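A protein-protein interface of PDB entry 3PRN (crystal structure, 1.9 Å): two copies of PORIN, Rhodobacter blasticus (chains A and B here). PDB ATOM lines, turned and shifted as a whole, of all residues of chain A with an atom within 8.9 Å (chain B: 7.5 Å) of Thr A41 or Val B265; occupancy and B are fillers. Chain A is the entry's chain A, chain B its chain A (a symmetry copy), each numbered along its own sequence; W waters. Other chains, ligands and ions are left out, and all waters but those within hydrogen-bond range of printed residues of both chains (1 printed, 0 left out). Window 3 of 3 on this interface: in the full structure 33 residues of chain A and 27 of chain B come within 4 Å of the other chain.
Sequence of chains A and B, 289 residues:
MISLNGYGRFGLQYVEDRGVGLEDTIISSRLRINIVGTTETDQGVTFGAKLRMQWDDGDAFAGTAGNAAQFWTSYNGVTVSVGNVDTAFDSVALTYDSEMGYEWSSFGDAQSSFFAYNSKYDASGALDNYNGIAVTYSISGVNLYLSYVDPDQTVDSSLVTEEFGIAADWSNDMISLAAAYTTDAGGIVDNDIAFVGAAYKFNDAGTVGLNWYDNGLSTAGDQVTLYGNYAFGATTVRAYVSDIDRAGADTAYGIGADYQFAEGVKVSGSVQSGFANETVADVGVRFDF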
ATOM      1  N   THR A  38      -2.258 -19.754   0.482  1.00  0.00           N
ATOM      2  CA  THR A  38      -3.585 -19.836  -0.128  1.00  0.00           C
ATOM      3  C   THR A  38      -4.674 -19.515   0.921  1.00  0.00           C
ATOM      4  O   THR A  38      -4.550 -19.821   2.080  1.00  0.00           O
ATOM      5  CB  THR A  38      -3.960 -21.228  -0.691  1.00  0.00           C
ATOM      6  OG1 THR A  38      -3.856 -22.195   0.347  1.00  0.00           O
ATOM      7  CG2 THR A  38      -2.976 -21.663  -1.753  1.00  0.00           C
ATOM      8  N   THR A  39      -5.702 -18.835   0.436  1.00  0.00           N
ATOM      9  CA  THR A  39      -6.834 -18.439   1.251  1.00  0.00           C
ATOM     10  C   THR A  39      -8.068 -18.982   0.490  1.00  0.00           C
ATOM     11  O   THR A  39      -8.349 -18.518  -0.619  1.00  0.00           O
ATOM     12  CB  THR A  39      -6.927 -16.896   1.330  1.00  0.00           C
ATOM     13  OG1 THR A  39      -5.650 -16.358   1.807  1.00  0.00           O
ATOM     14  CG2 THR A  39      -8.011 -16.460   2.304  1.00  0.00           C
ATOM     15  N   GLU A  40      -8.729 -19.939   1.061  1.00  0.00           N
ATOM     16  CA  GLU A  40      -9.948 -20.509   0.451  1.00  0.00           C
ATOM     17  C   GLU A  40     -11.141 -19.762   1.018  1.00  0.00           C
ATOM     18  O   GLU A  40     -11.035 -19.141   2.115  1.00  0.00           O
ATOM     19  CB  GLU A  40      -9.981 -21.991   0.868  1.00  0.00           C
ATOM     20  CG  GLU A  40      -8.879 -22.742   0.088  1.00  0.00           C
ATOM     21  CD  GLU A  40      -8.730 -24.179   0.582  1.00  0.00           C
ATOM     22  OE1 GLU A  40      -9.515 -24.690   1.424  1.00  0.00           O
ATOM     23  OE2 GLU A  40      -7.748 -24.852   0.102  1.00  0.00           O
ATOM     24  N   THR A  41     -12.248 -19.619   0.301  1.00  0.00           N
ATOM     25  CA  THR A  41     -13.394 -18.889   0.800  1.00  0.00           C
ATOM     26  C   THR A  41     -14.645 -19.815   0.618  1.00  0.00           C
ATOM     27  O   THR A  41     -14.630 -20.690  -0.224  1.00  0.00           O
ATOM     28  CB  THR A  41     -13.708 -17.580   0.071  1.00  0.00           C
ATOM     29  OG1 THR A  41     -13.998 -17.843  -1.311  1.00  0.00           O
ATOM     30  CG2 THR A  41     -12.486 -16.621   0.138  1.00  0.00           C
ATOM     31  N   ASP A  42     -15.694 -19.517   1.357  1.00  0.00           N
ATOM     32  CA  ASP A  42     -16.870 -20.403   1.221  1.00  0.00           C
ATOM     33  C   ASP A  42     -17.613 -20.074  -0.062  1.00  0.00           C
ATOM     34  O   ASP A  42     -18.472 -20.857  -0.443  1.00  0.00           O
ATOM     35  CB  ASP A  42     -17.686 -20.434   2.476  1.00  0.00           C
ATOM     36  CG  ASP A  42     -18.208 -19.091   2.912  1.00  0.00           C
ATOM     37  OD1 ASP A  42     -18.337 -18.148   2.107  1.00  0.00           O
ATOM     38  OD2 ASP A  42     -18.473 -18.929   4.111  1.00  0.00           O
ATOM     39  N   GLN A  43     -17.253 -18.981  -0.718  1.00  0.00           N
ATOM     40  CA  GLN A  43     -17.891 -18.627  -1.974  1.00  0.00           C
ATOM     41  C   GLN A  43     -17.265 -19.475  -3.079  1.00  0.00           C
ATOM     42  O   GLN A  43     -17.667 -19.406  -4.232  1.00  0.00           O
ATOM     43  CB  GLN A  43     -17.646 -17.138  -2.262  1.00  0.00           C
ATOM     44  CG  GLN A  43     -17.923 -16.267  -1.048  1.00  0.00           C
ATOM     45  CD  GLN A  43     -19.408 -16.203  -0.759  1.00  0.00           C
ATOM     46  OE1 GLN A  43     -20.193 -16.058  -1.696  1.00  0.00           O
ATOM     47  NE2 GLN A  43     -19.849 -16.314   0.474  1.00  0.00           N
ATOM     48  N   GLY A  44     -16.212 -20.250  -2.786  1.00  0.00           N
ATOM     49  CA  GLY A  44     -15.584 -21.053  -3.841  1.00  0.00           C
ATOM     50  C   GLY A  44     -14.479 -20.299  -4.611  1.00  0.00           C
ATOM     51  O   GLY A  44     -14.067 -20.778  -5.695  1.00  0.00           O
ATOM     52  N   VAL A  45     -14.103 -19.100  -4.207  1.00  0.00           N
ATOM     53  CA  VAL A  45     -13.017 -18.353  -4.854  1.00  0.00           C
ATOM     54  C   VAL A  45     -11.747 -18.615  -4.059  1.00  0.00           C
ATOM     55  O   VAL A  45     -11.807 -18.412  -2.842  1.00  0.00           O
ATOM     56  CB  VAL A  45     -13.297 -16.839  -4.832  1.00  0.00           C
ATOM     57  CG1 VAL A  45     -12.181 -16.089  -5.577  1.00  0.00           C
ATOM     58  CG2 VAL A  45     -14.648 -16.605  -5.517  1.00  0.00           C
ATOM     59  N   THR A  46     -10.680 -19.097  -4.651  1.00  0.00           N
ATOM     60  CA  THR A  46      -9.439 -19.307  -3.913  1.00  0.00           C
ATOM     61  C   THR A  46      -8.460 -18.188  -4.308  1.00  0.00           C
ATOM     62  O   THR A  46      -8.399 -17.829  -5.485  1.00  0.00           O
ATOM     63  CB  THR A  46      -8.825 -20.661  -4.322  1.00  0.00           C
ATOM     64  OG1 THR A  46      -9.715 -21.669  -3.844  1.00  0.00           O
ATOM     65  CG2 THR A  46      -7.460 -20.872  -3.658  1.00  0.00           C
ATOM     66  N   PHE A  47      -7.727 -17.649  -3.364  1.00  0.00           N
ATOM     67  CA  PHE A  47      -6.685 -16.666  -3.579  1.00  0.00           C
ATOM     68  C   PHE A  47      -5.345 -17.333  -3.214  1.00  0.00           C
ATOM     69  O   PHE A  47      -5.292 -18.104  -2.259  1.00  0.00           O
ATOM     70  CB  PHE A  47      -6.806 -15.377  -2.775  1.00  0.00           C
ATOM     71  CG  PHE A  47      -8.072 -14.623  -3.128  1.00  0.00           C
ATOM     72  CD1 PHE A  47      -9.278 -15.008  -2.574  1.00  0.00           C
ATOM     73  CD2 PHE A  47      -8.021 -13.548  -4.020  1.00  0.00           C
ATOM     74  CE1 PHE A  47     -10.442 -14.305  -2.915  1.00  0.00           C
ATOM     75  CE2 PHE A  47      -9.167 -12.848  -4.331  1.00  0.00           C
ATOM     76  CZ  PHE A  47     -10.388 -13.238  -3.781  1.00  0.00           C
ATOM     77  N   GLY A  48      -4.314 -17.065  -3.999  1.00  0.00           N
ATOM     78  CA  GLY A  48      -3.015 -17.658  -3.709  1.00  0.00           C
ATOM     79  C   GLY A  48      -1.871 -16.723  -4.083  1.00  0.00           C
ATOM     80  O   GLY A  48      -1.962 -15.785  -4.892  1.00  0.00           O
ATOM     81  N   THR A  73      -6.154 -15.813  -8.546  1.00  0.00           N
ATOM     82  CA  THR A  73      -7.498 -15.966  -8.035  1.00  0.00           C
ATOM     83  C   THR A  73      -8.165 -17.024  -8.949  1.00  0.00           C
ATOM     84  O   THR A  73      -7.985 -16.873 -10.187  1.00  0.00           O
ATOM     85  CB  THR A  73      -8.353 -14.700  -8.053  1.00  0.00           C
ATOM     86  OG1 THR A  73      -8.738 -14.409  -9.410  1.00  0.00           O
ATOM     87  CG2 THR A  73      -7.558 -13.506  -7.538  1.00  0.00           C
ATOM     88  N   SER A  74      -8.734 -18.055  -8.378  1.00  0.00           N
ATOM     89  CA  SER A  74      -9.365 -19.128  -9.099  1.00  0.00           C
ATOM     90  C   SER A  74     -10.827 -19.273  -8.706  1.00  0.00           C
ATOM     91  O   SER A  74     -11.187 -19.144  -7.527  1.00  0.00           O
ATOM     92  CB  SER A  74      -8.867 -20.556  -8.796  1.00  0.00           C
ATOM     93  OG  SER A  74      -7.530 -20.703  -9.250  1.00  0.00           O
ATOM     94  N   TYR A  75     -11.623 -19.573  -9.703  1.00  0.00           N
ATOM     95  CA  TYR A  75     -13.060 -19.756  -9.527  1.00  0.00           C
ATOM     96  C   TYR A  75     -13.635 -20.529 -10.720  1.00  0.00           C
ATOM     97  O   TYR A  75     -13.464 -20.095 -11.849  1.00  0.00           O
ATOM     98  CB  TYR A  75     -13.739 -18.393  -9.462  1.00  0.00           C
ATOM     99  CG  TYR A  75     -15.244 -18.510  -9.285  1.00  0.00           C
ATOM    100  CD1 TYR A  75     -15.752 -19.154  -8.159  1.00  0.00           C
ATOM    101  CD2 TYR A  75     -16.104 -17.978 -10.249  1.00  0.00           C
ATOM    102  CE1 TYR A  75     -17.129 -19.270  -7.989  1.00  0.00           C
ATOM    103  CE2 TYR A  75     -17.486 -18.093 -10.079  1.00  0.00           C
ATOM    104  CZ  TYR A  75     -17.998 -18.740  -8.949  1.00  0.00           C
ATOM    105  OH  TYR A  75     -19.340 -18.854  -8.781  1.00  0.00           O
ATOM    106  N   TYR B 259     -14.729  -3.804   1.640  1.00  0.00           N
ATOM    107  CA  TYR B 259     -15.753  -4.851   1.545  1.00  0.00           C
ATOM    108  C   TYR B 259     -15.123  -6.175   2.017  1.00  0.00           C
ATOM    109  O   TYR B 259     -14.120  -6.615   1.439  1.00  0.00           O
ATOM    110  CB  TYR B 259     -16.247  -4.907   0.114  1.00  0.00           C
ATOM    111  CG  TYR B 259     -17.287  -6.005  -0.047  1.00  0.00           C
ATOM    112  CD1 TYR B 259     -18.526  -5.734   0.543  1.00  0.00           C
ATOM    113  CD2 TYR B 259     -17.096  -7.203  -0.686  1.00  0.00           C
ATOM    114  CE1 TYR B 259     -19.564  -6.645   0.471  1.00  0.00           C
ATOM    115  CE2 TYR B 259     -18.131  -8.133  -0.744  1.00  0.00           C
ATOM    116  CZ  TYR B 259     -19.345  -7.841  -0.163  1.00  0.00           C
ATOM    117  OH  TYR B 259     -20.414  -8.712  -0.174  1.00  0.00           O
ATOM    118  N   GLN B 260     -15.717  -6.747   3.038  1.00  0.00           N
ATOM    119  CA  GLN B 260     -15.259  -8.020   3.623  1.00  0.00           C
ATOM    120  C   GLN B 260     -15.882  -9.155   2.817  1.00  0.00           C
ATOM    121  O   GLN B 260     -16.996  -9.602   3.086  1.00  0.00           O
ATOM    122  CB  GLN B 260     -15.602  -8.108   5.086  1.00  0.00           C
ATOM    123  CG  GLN B 260     -14.837  -9.118   5.927  1.00  0.00           C
ATOM    124  CD  GLN B 260     -13.360  -8.838   6.122  1.00  0.00           C
ATOM    125  OE1 GLN B 260     -12.943  -7.713   6.458  1.00  0.00           O
ATOM    126  NE2 GLN B 260     -12.469  -9.826   5.921  1.00  0.00           N
ATOM    127  N   PHE B 261     -15.187  -9.612   1.821  1.00  0.00           N
ATOM    128  CA  PHE B 261     -15.625 -10.661   0.926  1.00  0.00           C
ATOM    129  C   PHE B 261     -15.743 -12.005   1.646  1.00  0.00           C
ATOM    130  O   PHE B 261     -16.684 -12.765   1.357  1.00  0.00           O
ATOM    131  CB  PHE B 261     -14.700 -10.715  -0.277  1.00  0.00           C
ATOM    132  CG  PHE B 261     -15.020 -11.813  -1.258  1.00  0.00           C
ATOM    133  CD1 PHE B 261     -16.089 -11.680  -2.141  1.00  0.00           C
ATOM    134  CD2 PHE B 261     -14.294 -12.972  -1.305  1.00  0.00           C
ATOM    135  CE1 PHE B 261     -16.398 -12.698  -3.049  1.00  0.00           C
ATOM    136  CE2 PHE B 261     -14.578 -13.988  -2.182  1.00  0.00           C
ATOM    137  CZ  PHE B 261     -15.625 -13.849  -3.080  1.00  0.00           C
ATOM    138  N   ALA B 262     -14.830 -12.268   2.560  1.00  0.00           N
ATOM    139  CA  ALA B 262     -14.860 -13.537   3.309  1.00  0.00           C
ATOM    140  C   ALA B 262     -13.892 -13.377   4.449  1.00  0.00           C
ATOM    141  O   ALA B 262     -13.209 -12.317   4.492  1.00  0.00           O
ATOM    142  CB  ALA B 262     -14.518 -14.733   2.410  1.00  0.00           C
ATOM    143  N   GLU B 263     -13.829 -14.306   5.375  1.00  0.00           N
ATOM    144  CA  GLU B 263     -12.871 -14.183   6.460  1.00  0.00           C
ATOM    145  C   GLU B 263     -11.462 -14.079   5.804  1.00  0.00           C
ATOM    146  O   GLU B 263     -11.170 -14.905   4.901  1.00  0.00           O
ATOM    147  CB  GLU B 263     -12.968 -15.427   7.343  1.00  0.00           C
ATOM    148  CG  GLU B 263     -12.057 -15.319   8.552  1.00  0.00           C
ATOM    149  CD  GLU B 263     -12.021 -16.553   9.446  1.00  0.00           C
ATOM    150  OE1 GLU B 263     -13.013 -17.357   9.496  1.00  0.00           O
ATOM    151  OE2 GLU B 263     -10.958 -16.724  10.142  1.00  0.00           O
ATOM    152  N   GLY B 264     -10.634 -13.148   6.197  1.00  0.00           N
ATOM    153  CA  GLY B 264      -9.318 -13.054   5.593  1.00  0.00           C
ATOM    154  C   GLY B 264      -9.238 -12.509   4.154  1.00  0.00           C
ATOM    155  O   GLY B 264      -8.147 -12.424   3.571  1.00  0.00           O
ATOM    156  N   VAL B 265     -10.345 -12.148   3.535  1.00  0.00           N
ATOM    157  CA  VAL B 265     -10.267 -11.545   2.181  1.00  0.00           C
ATOM    158  C   VAL B 265     -10.963 -10.175   2.172  1.00  0.00           C
ATOM    159  O   VAL B 265     -12.180 -10.086   2.449  1.00  0.00           O
ATOM    160  CB  VAL B 265     -10.893 -12.406   1.089  1.00  0.00           C
ATOM    161  CG1 VAL B 265     -10.793 -11.741  -0.296  1.00  0.00           C
ATOM    162  CG2 VAL B 265     -10.215 -13.768   0.940  1.00  0.00           C
ATOM    163  N   LYS B 266     -10.201  -9.108   1.887  1.00  0.00           N
ATOM    164  CA  LYS B 266     -10.850  -7.781   1.955  1.00  0.00           C
ATOM    165  C   LYS B 266     -10.625  -6.989   0.702  1.00  0.00           C
ATOM    166  O   LYS B 266      -9.472  -6.946   0.212  1.00  0.00           O
ATOM    167  CB  LYS B 266     -10.320  -7.114   3.230  1.00  0.00           C
ATOM    168  CG  LYS B 266     -10.524  -5.640   3.284  1.00  0.00           C
ATOM    169  CD  LYS B 266     -10.686  -5.169   4.710  1.00  0.00           C
ATOM    170  CE  LYS B 266      -9.348  -4.788   5.309  1.00  0.00           C
ATOM    171  NZ  LYS B 266      -9.495  -4.941   6.816  1.00  0.00           N
ATOM    172  N   VAL B 267     -11.679  -6.422   0.083  1.00  0.00           N
ATOM    173  CA  VAL B 267     -11.499  -5.607  -1.138  1.00  0.00           C
ATOM    174  C   VAL B 267     -11.561  -4.135  -0.718  1.00  0.00           C
ATOM    175  O   VAL B 267     -12.445  -3.807   0.109  1.00  0.00           O
ATOM    176  CB  VAL B 267     -12.605  -5.859  -2.136  1.00  0.00           C
ATOM    177  CG1 VAL B 267     -12.413  -5.110  -3.461  1.00  0.00           C
ATOM    178  CG2 VAL B 267     -12.596  -7.364  -2.441  1.00  0.00           C
ATOM    179  N   VAL B 285      -7.321  -6.000  -3.650  1.00  0.00           N
ATOM    180  CA  VAL B 285      -7.649  -7.062  -2.683  1.00  0.00           C
ATOM    181  C   VAL B 285      -6.446  -7.451  -1.854  1.00  0.00           C
ATOM    182  O   VAL B 285      -5.314  -7.465  -2.339  1.00  0.00           O
ATOM    183  CB  VAL B 285      -8.000  -8.397  -3.355  1.00  0.00           C
ATOM    184  CG1 VAL B 285      -9.248  -9.058  -2.770  1.00  0.00           C
ATOM    185  CG2 VAL B 285      -8.233  -8.289  -4.854  1.00  0.00           C
ATOM    186  N   ARG B 286      -6.732  -7.762  -0.627  1.00  0.00           N
ATOM    187  CA  ARG B 286      -5.736  -8.310   0.280  1.00  0.00           C
ATOM    188  C   ARG B 286      -6.324  -9.654   0.781  1.00  0.00           C
ATOM    189  O   ARG B 286      -7.509  -9.732   1.168  1.00  0.00           O
ATOM    190  CB  ARG B 286      -5.475  -7.378   1.450  1.00  0.00           C
ATOM    191  CG  ARG B 286      -4.525  -8.003   2.470  1.00  0.00           C
ATOM    192  CD  ARG B 286      -4.462  -7.220   3.772  1.00  0.00           C
ATOM    193  NE  ARG B 286      -3.978  -8.019   4.902  1.00  0.00           N
ATOM    194  CZ  ARG B 286      -3.129  -7.556   5.822  1.00  0.00           C
ATOM    195  NH1 ARG B 286      -2.659  -6.303   5.750  1.00  0.00           N
ATOM    196  NH2 ARG B 286      -2.688  -8.273   6.861  1.00  0.00           N
ATOM    197  N   PHE B 287      -5.509 -10.680   0.860  1.00  0.00           N
ATOM    198  CA  PHE B 287      -5.908 -11.958   1.389  1.00  0.00           C
ATOM    199  C   PHE B 287      -4.821 -12.434   2.379  1.00  0.00           C
ATOM    200  O   PHE B 287      -3.638 -12.364   2.099  1.00  0.00           O
ATOM    201  CB  PHE B 287      -6.193 -12.971   0.304  1.00  0.00           C
ATOM    202  CG  PHE B 287      -5.105 -13.132  -0.738  1.00  0.00           C
ATOM    203  CD1 PHE B 287      -4.972 -12.240  -1.780  1.00  0.00           C
ATOM    204  CD2 PHE B 287      -4.206 -14.183  -0.615  1.00  0.00           C
ATOM    205  CE1 PHE B 287      -4.003 -12.438  -2.787  1.00  0.00           C
ATOM    206  CE2 PHE B 287      -3.225 -14.369  -1.588  1.00  0.00           C
ATOM    207  CZ  PHE B 287      -3.133 -13.504  -2.662  1.00  0.00           C
ATOM    208  N   ASP B 288      -5.251 -12.884   3.554  1.00  0.00           N
ATOM    209  CA  ASP B 288      -4.389 -13.280   4.629  1.00  0.00           C
ATOM    210  C   ASP B 288      -4.275 -14.809   4.639  1.00  0.00           C
ATOM    211  O   ASP B 288      -5.280 -15.465   4.333  1.00  0.00           O
ATOM    212  CB  ASP B 288      -4.967 -12.804   5.981  1.00  0.00           C
ATOM    213  CG  ASP B 288      -4.673 -11.315   6.113  1.00  0.00           C
ATOM    214  OD1 ASP B 288      -5.433 -10.460   5.521  1.00  0.00           O
ATOM    215  OD2 ASP B 288      -3.642 -10.919   6.772  1.00  0.00           O
HETATM  216  O   HOH W   1     -12.406 -17.608   3.992  1.00  0.00           O
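O of Asp B288 sits at hydrogen-bond distance from OG1 of Thr A39, 2.7 Å away.
The side-chain hydroxyl of Thr A41 lies close to the backbone NH of Gln A43 (3.5 Å).
The side-chain amide nitrogen (NE2) of Gln A43 is in hydrogen-bond range of the side-chain carboxylate (OD1) of Asp A42.
The backbone carbonyl oxygen (O) of Ala B262 lies within hydrogen-bond range of the side-chain amide nitrogen (NE2) of Gln B260 (3.0 Å).
The side-chain amide nitrogen (NE2) of Gln B260 lies within hydrogen-bond range of the backbone carbonyl oxygen (O) of Val B265.
O of Gly B264 sits at hydrogen-bond distance from N of Asp B288, 2.9 Å away.
The guanidinium group of Arg B286 lies within salt-bridge range of the side-chain carboxylate of Asp B288 (2.8 Å).
Thr A39 touches Val B265 (CG2 to CG2, 3.7 Å).
OG1 of Thr A39 touches CD2 of Phe B287 (3.6 Å).
Phe B261 touches Thr A41 (CE2 to OG1, 3.99 Å).
CG2 of Thr A41 touches CB of Ala B262 (3.6 Å).
CG2 of Thr A41 touches CG2 of Val B265, at 3.7 Å.
CG of Gln A43 touches CZ of Phe B261, at 3.9 Å.
CG2 of Val A45 touches CZ of Phe B261 (3.8 Å).
Val B265 touches Phe A47 (CG1 to CE1, 3.7 Å).
CB of Phe A47 touches CG of Phe B287, at 3.5 Å.
Phe B287 touches Gly A48.
Printed residues of chain B within 4 Å of Thr A41: Phe B261 (3.99 Å), Ala B262 (3.6 Å) and Val B265 (3.7 Å).
Val B265 touches just these residues of chain A: Thr A39 (3.7 Å), Thr A41 (3.7 Å) and Phe A47 (3.7 Å).
Ala B262 touches just one residue of chain A: Thr A41.
No residue of chain A comes within 4 Å of Gly B264.
Printed residues of chain A within 4 Å of Phe B261: Thr A41, Gln A43 and Val A45.
Printed residues of chain B within 4 Å of Gln A43: Phe B261 (3.9 Å).
Lys B266 touches none of the printed residues of chain A.
Val B285 touches none of the printed residues of chain A.
The nearest residue of chain A that does not touch Val B265 is Glu A40 (5.6 Å).
Hydrophobic or aromatic side chains of chain A within 4 Å of the printed part of chain B: Val A45 and Phe A47.
Among the printed residues, 11 pairs touch across the chains.
No position is printed for both chains.
Water W1 lies within hydrogen-bond range of O of Glu A40 and O of Glu B263.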
